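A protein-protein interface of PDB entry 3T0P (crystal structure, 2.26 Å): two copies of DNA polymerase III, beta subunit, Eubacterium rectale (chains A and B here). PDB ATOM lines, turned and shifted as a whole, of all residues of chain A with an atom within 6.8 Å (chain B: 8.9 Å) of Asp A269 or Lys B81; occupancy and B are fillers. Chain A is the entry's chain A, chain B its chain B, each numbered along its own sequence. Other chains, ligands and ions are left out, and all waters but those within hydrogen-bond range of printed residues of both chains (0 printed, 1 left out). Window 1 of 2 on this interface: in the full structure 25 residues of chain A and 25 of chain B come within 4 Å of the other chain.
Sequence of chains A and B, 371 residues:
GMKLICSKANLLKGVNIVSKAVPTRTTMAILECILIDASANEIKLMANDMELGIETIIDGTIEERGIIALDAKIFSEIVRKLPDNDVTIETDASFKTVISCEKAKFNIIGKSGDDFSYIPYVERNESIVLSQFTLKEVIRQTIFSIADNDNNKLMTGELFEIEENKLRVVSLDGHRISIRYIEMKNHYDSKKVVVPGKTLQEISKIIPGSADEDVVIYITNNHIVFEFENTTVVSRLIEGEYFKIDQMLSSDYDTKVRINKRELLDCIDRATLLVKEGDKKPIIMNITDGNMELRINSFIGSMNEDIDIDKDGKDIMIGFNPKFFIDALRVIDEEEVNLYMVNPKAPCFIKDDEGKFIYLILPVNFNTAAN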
ATOM      1  N   LEU A 264     -24.696  30.760  20.424  1.00  0.00           N
ATOM      2  CA  LEU A 264     -25.201  31.310  19.168  1.00  0.00           C
ATOM      3  C   LEU A 264     -24.035  31.743  18.286  1.00  0.00           C
ATOM      4  O   LEU A 264     -23.964  31.346  17.118  1.00  0.00           O
ATOM      5  CB  LEU A 264     -26.203  32.478  19.402  1.00  0.00           C
ATOM      6  CG  LEU A 264     -26.873  33.040  18.131  1.00  0.00           C
ATOM      7  CD1 LEU A 264     -27.597  31.937  17.324  1.00  0.00           C
ATOM      8  CD2 LEU A 264     -27.839  34.175  18.463  1.00  0.00           C
ATOM      9  N   LEU A 265     -23.104  32.495  18.851  1.00  0.00           N
ATOM     10  CA  LEU A 265     -21.900  32.957  18.155  1.00  0.00           C
ATOM     11  C   LEU A 265     -21.099  31.783  17.586  1.00  0.00           C
ATOM     12  O   LEU A 265     -20.791  31.789  16.388  1.00  0.00           O
ATOM     13  CB  LEU A 265     -21.011  33.817  19.084  1.00  0.00           C
ATOM     14  CG  LEU A 265     -19.663  34.299  18.517  1.00  0.00           C
ATOM     15  CD1 LEU A 265     -19.828  35.008  17.165  1.00  0.00           C
ATOM     16  CD2 LEU A 265     -18.976  35.194  19.505  1.00  0.00           C
ATOM     17  N   ASP A 266     -20.794  30.769  18.404  1.00  0.00           N
ATOM     18  CA  ASP A 266     -20.037  29.594  17.907  1.00  0.00           C
ATOM     19  C   ASP A 266     -20.756  28.845  16.774  1.00  0.00           C
ATOM     20  O   ASP A 266     -20.104  28.392  15.833  1.00  0.00           O
ATOM     21  CB  ASP A 266     -19.725  28.620  19.047  1.00  0.00           C
ATOM     22  CG  ASP A 266     -18.641  29.141  19.986  1.00  0.00           C
ATOM     23  OD1 ASP A 266     -18.065  30.220  19.693  1.00  0.00           O
ATOM     24  OD2 ASP A 266     -18.398  28.498  21.034  1.00  0.00           O
ATOM     25  N   CYS A 267     -22.084  28.760  16.834  1.00  0.00           N
ATOM     26  CA  CYS A 267     -22.826  28.068  15.817  1.00  0.00           C
ATOM     27  C   CYS A 267     -22.827  28.836  14.486  1.00  0.00           C
ATOM     28  O   CYS A 267     -22.680  28.222  13.434  1.00  0.00           O
ATOM     29  CB  CYS A 267     -24.250  27.805  16.280  1.00  0.00           C
ATOM     30  SG  CYS A 267     -25.334  27.336  14.916  1.00  0.00           S
ATOM     31  N   ILE A 268     -23.084  30.150  14.523  1.00  0.00           N
ATOM     32  CA  ILE A 268     -23.125  30.986  13.312  1.00  0.00           C
ATOM     33  C   ILE A 268     -21.700  31.033  12.696  1.00  0.00           C
ATOM     34  O   ILE A 268     -21.553  30.970  11.479  1.00  0.00           O
ATOM     35  CB  ILE A 268     -23.700  32.391  13.587  1.00  0.00           C
ATOM     36  CG1 ILE A 268     -25.121  32.255  14.177  1.00  0.00           C
ATOM     37  CG2 ILE A 268     -23.716  33.214  12.274  1.00  0.00           C
ATOM     38  CD1 ILE A 268     -25.873  33.556  14.470  1.00  0.00           C
ATOM     39  N   ASP A 269     -20.680  31.074  13.536  1.00  0.00           N
ATOM     40  CA  ASP A 269     -19.293  31.046  13.086  1.00  0.00           C
ATOM     41  C   ASP A 269     -19.000  29.698  12.372  1.00  0.00           C
ATOM     42  O   ASP A 269     -18.420  29.725  11.292  1.00  0.00           O
ATOM     43  CB  ASP A 269     -18.360  31.292  14.265  1.00  0.00           C
ATOM     44  CG  ASP A 269     -16.877  31.346  13.921  1.00  0.00           C
ATOM     45  OD1 ASP A 269     -16.503  32.130  13.022  1.00  0.00           O
ATOM     46  OD2 ASP A 269     -16.086  30.636  14.592  1.00  0.00           O
ATOM     47  N   ARG A 270     -19.479  28.558  12.914  1.00  0.00           N
ATOM     48  CA  ARG A 270     -19.336  27.225  12.293  1.00  0.00           C
ATOM     49  C   ARG A 270     -19.945  27.220  10.899  1.00  0.00           C
ATOM     50  O   ARG A 270     -19.326  26.738   9.967  1.00  0.00           O
ATOM     51  CB  ARG A 270     -20.043  26.133  13.129  1.00  0.00           C
ATOM     52  CG  ARG A 270     -19.179  25.545  14.191  1.00  0.00           C
ATOM     53  CD  ARG A 270     -19.796  24.324  14.828  1.00  0.00           C
ATOM     54  NE  ARG A 270     -20.788  24.660  15.855  1.00  0.00           N
ATOM     55  CZ  ARG A 270     -20.494  25.029  17.101  1.00  0.00           C
ATOM     56  NH1 ARG A 270     -19.232  25.142  17.488  1.00  0.00           N
ATOM     57  NH2 ARG A 270     -21.462  25.300  17.963  1.00  0.00           N
ATOM     58  N   ALA A 271     -21.167  27.738  10.771  1.00  0.00           N
ATOM     59  CA  ALA A 271     -21.887  27.833   9.509  1.00  0.00           C
ATOM     60  C   ALA A 271     -21.093  28.606   8.423  1.00  0.00           C
ATOM     61  O   ALA A 271     -21.142  28.216   7.263  1.00  0.00           O
ATOM     62  CB  ALA A 271     -23.222  28.511   9.740  1.00  0.00           C
ATOM     63  N   THR A 272     -20.355  29.653   8.789  1.00  0.00           N
ATOM     64  CA  THR A 272     -19.626  30.454   7.801  1.00  0.00           C
ATOM     65  C   THR A 272     -18.530  29.686   7.066  1.00  0.00           C
ATOM     66  O   THR A 272     -18.233  30.049   5.924  1.00  0.00           O
ATOM     67  CB  THR A 272     -19.057  31.725   8.390  1.00  0.00           C
ATOM     68  OG1 THR A 272     -18.106  31.412   9.401  1.00  0.00           O
ATOM     69  CG2 THR A 272     -20.136  32.638   8.914  1.00  0.00           C
ATOM     70  N   LEU A 273     -17.984  28.595   7.647  1.00  0.00           N
ATOM     71  CA  LEU A 273     -16.946  27.839   6.950  1.00  0.00           C
ATOM     72  C   LEU A 273     -17.509  27.234   5.617  1.00  0.00           C
ATOM     73  O   LEU A 273     -16.742  26.943   4.707  1.00  0.00           O
ATOM     74  CB  LEU A 273     -16.323  26.747   7.862  1.00  0.00           C
ATOM     75  CG  LEU A 273     -17.124  25.456   8.174  1.00  0.00           C
ATOM     76  CD1 LEU A 273     -16.947  24.402   7.090  1.00  0.00           C
ATOM     77  CD2 LEU A 273     -16.714  24.881   9.516  1.00  0.00           C
ATOM     78  N   LEU A 274     -18.835  27.057   5.514  1.00  0.00           N
ATOM     79  CA  LEU A 274     -19.435  26.491   4.304  1.00  0.00           C
ATOM     80  C   LEU A 274     -19.640  27.534   3.178  1.00  0.00           C
ATOM     81  O   LEU A 274     -19.911  27.141   2.049  1.00  0.00           O
ATOM     82  CB  LEU A 274     -20.755  25.798   4.637  1.00  0.00           C
ATOM     83  CG  LEU A 274     -20.635  24.524   5.453  1.00  0.00           C
ATOM     84  CD1 LEU A 274     -21.974  24.051   5.893  1.00  0.00           C
ATOM     85  CD2 LEU A 274     -19.943  23.406   4.670  1.00  0.00           C
ATOM     86  N   LYS A 276     -17.758  30.350   0.962  1.00  0.00           N
ATOM     87  CA  LYS A 276     -16.435  30.866   0.565  1.00  0.00           C
ATOM     88  C   LYS A 276     -16.493  31.743  -0.684  1.00  0.00           C
ATOM     89  O   LYS A 276     -17.275  31.459  -1.598  1.00  0.00           O
ATOM     90  CB  LYS A 276     -15.441  29.706   0.301  1.00  0.00           C
ATOM     91  CG  LYS A 276     -15.303  28.667   1.419  1.00  0.00           C
ATOM     92  CD  LYS A 276     -14.449  29.093   2.608  1.00  0.00           C
ATOM     93  CE  LYS A 276     -13.939  27.867   3.322  1.00  0.00           C
ATOM     94  NZ  LYS A 276     -13.881  28.059   4.790  1.00  0.00           N
ATOM     95  N   ILE A 283     -28.000  32.165   6.670  1.00  0.00           N
ATOM     96  CA  ILE A 283     -28.194  31.184   7.729  1.00  0.00           C
ATOM     97  C   ILE A 283     -29.726  31.199   8.008  1.00  0.00           C
ATOM     98  O   ILE A 283     -30.306  32.279   8.099  1.00  0.00           O
ATOM     99  CB  ILE A 283     -27.301  31.426   8.986  1.00  0.00           C
ATOM    100  CG1 ILE A 283     -27.438  30.251   9.963  1.00  0.00           C
ATOM    101  CG2 ILE A 283     -27.576  32.782   9.683  1.00  0.00           C
ATOM    102  CD1 ILE A 283     -26.277  29.934  10.717  1.00  0.00           C
ATOM    103  N   MET A 303     -24.987  22.223   6.962  1.00  0.00           N
ATOM    104  CA  MET A 303     -24.877  22.174   8.405  1.00  0.00           C
ATOM    105  C   MET A 303     -26.251  22.237   9.024  1.00  0.00           C
ATOM    106  O   MET A 303     -27.108  22.981   8.552  1.00  0.00           O
ATOM    107  CB  MET A 303     -24.021  23.337   8.925  1.00  0.00           C
ATOM    108  CG  MET A 303     -23.673  23.177  10.391  1.00  0.00           C
ATOM    109  SD  MET A 303     -23.290  24.821  11.336  1.00  0.00           S
ATOM    110  CE  MET A 303     -22.783  23.906  12.838  1.00  0.00           C
ATOM    111  N   PRO A 322     -25.081  35.711   7.859  1.00  0.00           N
ATOM    112  CA  PRO A 322     -24.403  35.319   9.118  1.00  0.00           C
ATOM    113  C   PRO A 322     -23.420  36.375   9.640  1.00  0.00           C
ATOM    114  O   PRO A 322     -23.331  36.550  10.864  1.00  0.00           O
ATOM    115  CB  PRO A 322     -23.656  34.020   8.755  1.00  0.00           C
ATOM    116  CG  PRO A 322     -23.783  33.849   7.300  1.00  0.00           C
ATOM    117  CD  PRO A 322     -24.906  34.701   6.791  1.00  0.00           C
ATOM    118  N   ILE A 326     -22.567  37.666  13.550  1.00  0.00           N
ATOM    119  CA  ILE A 326     -21.192  37.442  13.985  1.00  0.00           C
ATOM    120  C   ILE A 326     -20.606  38.748  14.505  1.00  0.00           C
ATOM    121  O   ILE A 326     -20.104  38.785  15.630  1.00  0.00           O
ATOM    122  CB  ILE A 326     -20.324  36.847  12.822  1.00  0.00           C
ATOM    123  CG1 ILE A 326     -20.668  35.377  12.544  1.00  0.00           C
ATOM    124  CG2 ILE A 326     -18.824  37.018  13.069  1.00  0.00           C
ATOM    125  CD1 ILE A 326     -20.486  34.440  13.705  1.00  0.00           C
ATOM    126  N   ARG A 330     -19.913  39.157  18.556  1.00  0.00           N
ATOM    127  CA  ARG A 330     -18.482  39.305  18.949  1.00  0.00           C
ATOM    128  C   ARG A 330     -18.223  40.491  19.886  1.00  0.00           C
ATOM    129  O   ARG A 330     -17.199  40.500  20.558  1.00  0.00           O
ATOM    130  CB  ARG A 330     -17.579  39.499  17.728  1.00  0.00           C
ATOM    131  CG  ARG A 330     -17.221  38.224  17.036  1.00  0.00           C
ATOM    132  CD  ARG A 330     -16.225  38.538  15.942  1.00  0.00           C
ATOM    133  NE  ARG A 330     -15.799  37.326  15.250  1.00  0.00           N
ATOM    134  CZ  ARG A 330     -15.384  37.298  13.990  1.00  0.00           C
ATOM    135  NH1 ARG A 330     -15.358  38.412  13.266  1.00  0.00           N
ATOM    136  NH2 ARG A 330     -15.034  36.149  13.430  1.00  0.00           N
ATOM    137  N   LYS B   8     -12.319  15.912  20.132  1.00  0.00           N
ATOM    138  CA  LYS B   8     -12.056  17.027  19.230  1.00  0.00           C
ATOM    139  C   LYS B   8     -10.592  17.487  19.331  1.00  0.00           C
ATOM    140  O   LYS B   8      -9.995  17.805  18.307  1.00  0.00           O
ATOM    141  CB  LYS B   8     -13.030  18.198  19.523  1.00  0.00           C
ATOM    142  CG  LYS B   8     -12.825  19.470  18.678  1.00  0.00           C
ATOM    143  CD  LYS B   8     -11.903  20.476  19.381  1.00  0.00           C
ATOM    144  CE  LYS B   8     -11.700  21.779  18.661  1.00  0.00           C
ATOM    145  NZ  LYS B   8     -12.809  22.742  18.907  1.00  0.00           N
ATOM    146  N   LEU B  12      -8.054  17.665  16.359  1.00  0.00           N
ATOM    147  CA  LEU B  12      -7.528  18.968  15.990  1.00  0.00           C
ATOM    148  C   LEU B  12      -6.005  18.952  15.953  1.00  0.00           C
ATOM    149  O   LEU B  12      -5.417  19.450  14.993  1.00  0.00           O
ATOM    150  CB  LEU B  12      -8.048  20.092  16.916  1.00  0.00           C
ATOM    151  CG  LEU B  12      -7.505  21.491  16.636  1.00  0.00           C
ATOM    152  CD1 LEU B  12      -7.809  21.931  15.194  1.00  0.00           C
ATOM    153  CD2 LEU B  12      -8.039  22.515  17.650  1.00  0.00           C
ATOM    154  N   VAL B  15      -5.047  17.012  12.667  1.00  0.00           N
ATOM    155  CA  VAL B  15      -5.265  17.692  11.376  1.00  0.00           C
ATOM    156  C   VAL B  15      -4.270  18.846  11.234  1.00  0.00           C
ATOM    157  O   VAL B  15      -3.800  19.087  10.133  1.00  0.00           O
ATOM    158  CB  VAL B  15      -6.730  18.149  11.084  1.00  0.00           C
ATOM    159  CG1 VAL B  15      -7.730  17.024  11.333  1.00  0.00           C
ATOM    160  CG2 VAL B  15      -7.113  19.409  11.860  1.00  0.00           C
ATOM    161  N   ILE B  74     -11.572  22.258   4.387  1.00  0.00           N
ATOM    162  CA  ILE B  74     -12.904  22.124   4.979  1.00  0.00           C
ATOM    163  C   ILE B  74     -12.857  21.259   6.254  1.00  0.00           C
ATOM    164  O   ILE B  74     -13.409  21.670   7.263  1.00  0.00           O
ATOM    165  CB  ILE B  74     -13.951  21.594   3.956  1.00  0.00           C
ATOM    166  CG1 ILE B  74     -14.017  22.484   2.683  1.00  0.00           C
ATOM    167  CG2 ILE B  74     -15.344  21.434   4.589  1.00  0.00           C
ATOM    168  CD1 ILE B  74     -14.077  24.103   2.883  1.00  0.00           C
ATOM    169  N   PHE B  75     -12.184  20.101   6.216  1.00  0.00           N
ATOM    170  CA  PHE B  75     -12.120  19.206   7.359  1.00  0.00           C
ATOM    171  C   PHE B  75     -11.418  19.864   8.560  1.00  0.00           C
ATOM    172  O   PHE B  75     -11.939  19.777   9.659  1.00  0.00           O
ATOM    173  CB  PHE B  75     -11.461  17.880   6.976  1.00  0.00           C
ATOM    174  CG  PHE B  75     -11.338  16.878   8.087  1.00  0.00           C
ATOM    175  CD1 PHE B  75     -12.454  16.487   8.817  1.00  0.00           C
ATOM    176  CD2 PHE B  75     -10.131  16.255   8.345  1.00  0.00           C
ATOM    177  CE1 PHE B  75     -12.346  15.529   9.828  1.00  0.00           C
ATOM    178  CE2 PHE B  75     -10.026  15.290   9.343  1.00  0.00           C
ATOM    179  CZ  PHE B  75     -11.126  14.952  10.099  1.00  0.00           C
ATOM    180  N   SER B  76     -10.288  20.549   8.354  1.00  0.00           N
ATOM    181  CA  SER B  76      -9.607  21.220   9.455  1.00  0.00           C
ATOM    182  C   SER B  76     -10.464  22.358  10.035  1.00  0.00           C
ATOM    183  O   SER B  76     -10.543  22.490  11.254  1.00  0.00           O
ATOM    184  CB  SER B  76      -8.242  21.756   9.021  1.00  0.00           C
ATOM    185  OG  SER B  76      -8.358  22.551   7.859  1.00  0.00           O
ATOM    186  N   GLU B  77     -11.112  23.161   9.182  1.00  0.00           N
ATOM    187  CA  GLU B  77     -11.949  24.271   9.647  1.00  0.00           C
ATOM    188  C   GLU B  77     -13.151  23.720  10.425  1.00  0.00           C
ATOM    189  O   GLU B  77     -13.506  24.278  11.455  1.00  0.00           O
ATOM    190  CB  GLU B  77     -12.386  25.156   8.478  1.00  0.00           C
ATOM    191  CG  GLU B  77     -12.661  26.588   8.881  1.00  0.00           C
ATOM    192  CD  GLU B  77     -12.474  27.633   7.794  1.00  0.00           C
ATOM    193  OE1 GLU B  77     -11.460  27.549   7.061  1.00  0.00           O
ATOM    194  OE2 GLU B  77     -13.302  28.571   7.721  1.00  0.00           O
ATOM    195  N   ILE B  78     -13.708  22.563   9.999  1.00  0.00           N
ATOM    196  CA  ILE B  78     -14.824  21.932  10.713  1.00  0.00           C
ATOM    197  C   ILE B  78     -14.350  21.536  12.114  1.00  0.00           C
ATOM    198  O   ILE B  78     -14.952  21.970  13.085  1.00  0.00           O
ATOM    199  CB  ILE B  78     -15.444  20.731   9.950  1.00  0.00           C
ATOM    200  CG1 ILE B  78     -16.203  21.206   8.698  1.00  0.00           C
ATOM    201  CG2 ILE B  78     -16.361  19.885  10.855  1.00  0.00           C
ATOM    202  CD1 ILE B  78     -16.765  20.103   7.795  1.00  0.00           C
ATOM    203  N   VAL B  79     -13.232  20.791  12.203  1.00  0.00           N
ATOM    204  CA  VAL B  79     -12.682  20.235  13.439  1.00  0.00           C
ATOM    205  C   VAL B  79     -12.321  21.351  14.404  1.00  0.00           C
ATOM    206  O   VAL B  79     -12.661  21.270  15.581  1.00  0.00           O
ATOM    207  CB  VAL B  79     -11.498  19.270  13.143  1.00  0.00           C
ATOM    208  CG1 VAL B  79     -10.750  18.895  14.417  1.00  0.00           C
ATOM    209  CG2 VAL B  79     -11.998  18.013  12.436  1.00  0.00           C
ATOM    210  N   ARG B  80     -11.695  22.421  13.888  1.00  0.00           N
ATOM    211  CA  ARG B  80     -11.259  23.602  14.642  1.00  0.00           C
ATOM    212  C   ARG B  80     -12.429  24.423  15.226  1.00  0.00           C
ATOM    213  O   ARG B  80     -12.236  25.117  16.230  1.00  0.00           O
ATOM    214  CB  ARG B  80     -10.419  24.508  13.733  1.00  0.00           C
ATOM    215  CG  ARG B  80      -9.446  25.413  14.468  1.00  0.00           C
ATOM    216  CD  ARG B  80      -8.476  26.074  13.515  1.00  0.00           C
ATOM    217  NE  ARG B  80      -7.602  25.103  12.847  1.00  0.00           N
ATOM    218  CZ  ARG B  80      -7.564  24.927  11.532  1.00  0.00           C
ATOM    219  NH1 ARG B  80      -8.341  25.656  10.734  1.00  0.00           N
ATOM    220  NH2 ARG B  80      -6.736  24.038  11.002  1.00  0.00           N
ATOM    221  N   LYS B  81     -13.602  24.399  14.567  1.00  0.00           N
ATOM    222  CA  LYS B  81     -14.786  25.141  14.997  1.00  0.00           C
ATOM    223  C   LYS B  81     -15.851  24.290  15.708  1.00  0.00           C
ATOM    224  O   LYS B  81     -16.791  24.857  16.249  1.00  0.00           O
ATOM    225  CB  LYS B  81     -15.386  25.897  13.807  1.00  0.00           C
ATOM    226  CG  LYS B  81     -14.454  27.020  13.357  1.00  0.00           C
ATOM    227  CD  LYS B  81     -15.130  27.971  12.407  1.00  0.00           C
ATOM    228  CE  LYS B  81     -14.274  29.170  12.083  1.00  0.00           C
ATOM    229  NZ  LYS B  81     -14.810  29.867  10.888  1.00  0.00           N
ATOM    230  N   LEU B  82     -15.666  22.964  15.798  1.00  0.00           N
ATOM    231  CA  LEU B  82     -16.616  22.131  16.521  1.00  0.00           C
ATOM    232  C   LEU B  82     -16.488  22.339  18.027  1.00  0.00           C
ATOM    233  O   LEU B  82     -15.428  22.769  18.486  1.00  0.00           O
ATOM    234  CB  LEU B  82     -16.425  20.635  16.194  1.00  0.00           C
ATOM    235  CG  LEU B  82     -17.026  20.143  14.885  1.00  0.00           C
ATOM    236  CD1 LEU B  82     -16.691  18.688  14.655  1.00  0.00           C
ATOM    237  CD2 LEU B  82     -18.513  20.389  14.803  1.00  0.00           C
ATOM    238  N   PRO B  83     -17.557  22.059  18.810  1.00  0.00           N
ATOM    239  CA  PRO B  83     -17.423  22.147  20.283  1.00  0.00           C
ATOM    240  C   PRO B  83     -16.369  21.148  20.804  1.00  0.00           C
ATOM    241  O   PRO B  83     -16.000  20.195  20.095  1.00  0.00           O
ATOM    242  CB  PRO B  83     -18.830  21.769  20.797  1.00  0.00           C
ATOM    243  CG  PRO B  83     -19.728  21.755  19.620  1.00  0.00           C
ATOM    244  CD  PRO B  83     -18.896  21.567  18.405  1.00  0.00           C
ATOM    245  N   ASP B  84     -15.899  21.344  22.045  1.00  0.00           N
ATOM    246  CA  ASP B  84     -14.865  20.499  22.652  1.00  0.00           C
ATOM    247  C   ASP B  84     -15.489  19.281  23.281  1.00  0.00           C
ATOM    248  O   ASP B  84     -15.628  19.199  24.495  1.00  0.00           O
ATOM    249  CB  ASP B  84     -14.060  21.308  23.678  1.00  0.00           C
ATOM    250  CG  ASP B  84     -13.202  22.396  23.051  1.00  0.00           C
ATOM    251  OD1 ASP B  84     -13.177  22.499  21.798  1.00  0.00           O
ATOM    252  OD2 ASP B  84     -12.513  23.096  23.792  1.00  0.00           O
ATOM    253  N   VAL B  87     -16.239  13.846  18.643  1.00  0.00           N
ATOM    254  CA  VAL B  87     -16.599  14.058  17.256  1.00  0.00           C
ATOM    255  C   VAL B  87     -16.849  12.699  16.621  1.00  0.00           C
ATOM    256  O   VAL B  87     -15.993  11.818  16.705  1.00  0.00           O
ATOM    257  CB  VAL B  87     -15.491  14.849  16.516  1.00  0.00           C
ATOM    258  CG1 VAL B  87     -15.820  14.998  15.035  1.00  0.00           C
ATOM    259  CG2 VAL B  87     -15.273  16.219  17.162  1.00  0.00           C
ATOM    260  N   CYS B 101     -21.039  16.487  16.386  1.00  0.00           N
ATOM    261  CA  CYS B 101     -20.483  16.803  17.698  1.00  0.00           C
ATOM    262  C   CYS B 101     -21.525  17.566  18.465  1.00  0.00           C
ATOM    263  O   CYS B 101     -21.960  18.603  17.984  1.00  0.00           O
ATOM    264  CB  CYS B 101     -19.197  17.622  17.548  1.00  0.00           C
ATOM    265  SG  CYS B 101     -18.377  17.990  19.109  1.00  0.00           S
ATOM    266  N   ALA B 104     -24.504  19.658  16.849  1.00  0.00           N
ATOM    267  CA  ALA B 104     -24.101  20.173  15.548  1.00  0.00           C
ATOM    268  C   ALA B 104     -23.753  19.034  14.599  1.00  0.00           C
ATOM    269  O   ALA B 104     -23.213  17.999  15.011  1.00  0.00           O
ATOM    270  CB  ALA B 104     -22.927  21.117  15.713  1.00  0.00           C
ATOM    271  N   PHE B 106     -22.458  18.315  10.308  1.00  0.00           N
ATOM    272  CA  PHE B 106     -21.988  18.766   8.999  1.00  0.00           C
ATOM    273  C   PHE B 106     -22.131  17.662   7.991  1.00  0.00           C
ATOM    274  O   PHE B 106     -21.722  16.537   8.272  1.00  0.00           O
ATOM    275  CB  PHE B 106     -20.515  19.204   9.037  1.00  0.00           C
ATOM    276  CG  PHE B 106     -20.295  20.566   9.628  1.00  0.00           C
ATOM    277  CD1 PHE B 106     -20.368  21.703   8.833  1.00  0.00           C
ATOM    278  CD2 PHE B 106     -20.053  20.720  10.990  1.00  0.00           C
ATOM    279  CE1 PHE B 106     -20.191  22.961   9.384  1.00  0.00           C
ATOM    280  CE2 PHE B 106     -19.873  21.980  11.544  1.00  0.00           C
ATOM    281  CZ  PHE B 106     -19.914  23.093  10.733  1.00  0.00           C
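The backbone carbonyl oxygen of Pro B83 is in hydrogen-bond range of the side-chain sulfur of Cys B101, at 3.4 Å. SD of Met A303 lies within hydrogen-bond range of N of Ala A271, 3.7 Å away. The backbone carbonyl oxygen (O) of Leu B82 lies within hydrogen-bond range of the side-chain amino group (NZ) of Lys B8 (2.7 Å). The side-chain carboxylate (OE2) of Glu B77 lies within salt-bridge range of the side-chain amino group (NZ) of Lys B81 (3.7 Å). NZ of Lys A276 is in hydrogen-bond range of O of Leu A273 (3.1 Å). The side-chain hydroxyl (OG1) of Thr A272 is in hydrogen-bond range of the backbone carbonyl oxygen (O) of Asp A269 (2.6 Å).
Printed residues of chain A that touch a printed residue of chain B: Asp A269, Arg A270, Thr A272, Leu A273, Lys A276 and Met A303. Among the printed residues, 12 pairs touch across the chains. Among the printed residues, Asp or Glu carboxylates within 4 Å of a Lys or Arg side-chain nitrogen of the other chain: Asp A269 with Lys B81 and Lys A276 with Glu B77.
Cys A267 touches none of the printed residues of chain B. Asp A269 touches one residue of chain B. Arg A330 touches none of the printed residues of chain B. Of the printed residues of chain A, Glu B77 touches Leu A273 (3.5 Å) and Lys A276 (3.0 Å). Of chain A, only Asp A269 (3.4 Å), Arg A270 (2.8 Å) and Thr A272 (3.9 Å) come within 4 Å of Lys B81. Of the printed residues of chain A, Pro B83 touches Arg A270 (3.7 Å). The nearest residue of chain A that does not touch Lys B81 is Leu A273 (4.5 Å).
No position is printed for both chains. Of the 12 pairs that touch across the chains among the printed residues, none has its exchanged pair printed and touching as well.
The side-chain carboxylate of Glu B77 lies within salt-bridge range of the side-chain amino group of Lys A276 (3.0 Å). The side-chain carboxylate (OD1) of Asp A269 lies within salt-bridge range of the side-chain amino group (NZ) of Lys B81 (3.5 Å). The guanidinium group of Arg A270 lies within hydrogen-bond range of the backbone carbonyl oxygen of Lys B81 (2.8 Å).
Among the printed residues, pairs that only touch across the chains: Arg A270 with Leu B82 (3.96 Å), Arg A270 with Pro B83 (3.7 Å), Arg A270 with Phe B106 (3.8 Å), Thr A272 with Lys B81 (3.9 Å), Leu A273 with Glu B77 (3.5 Å), Leu A273 with Ile B78 (3.7 Å), Leu A273 with Phe B106 (3.9 Å), Lys A276 with Ile B74 (3.8 Å) and Met A303 with Phe B106 (3.6 Å).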
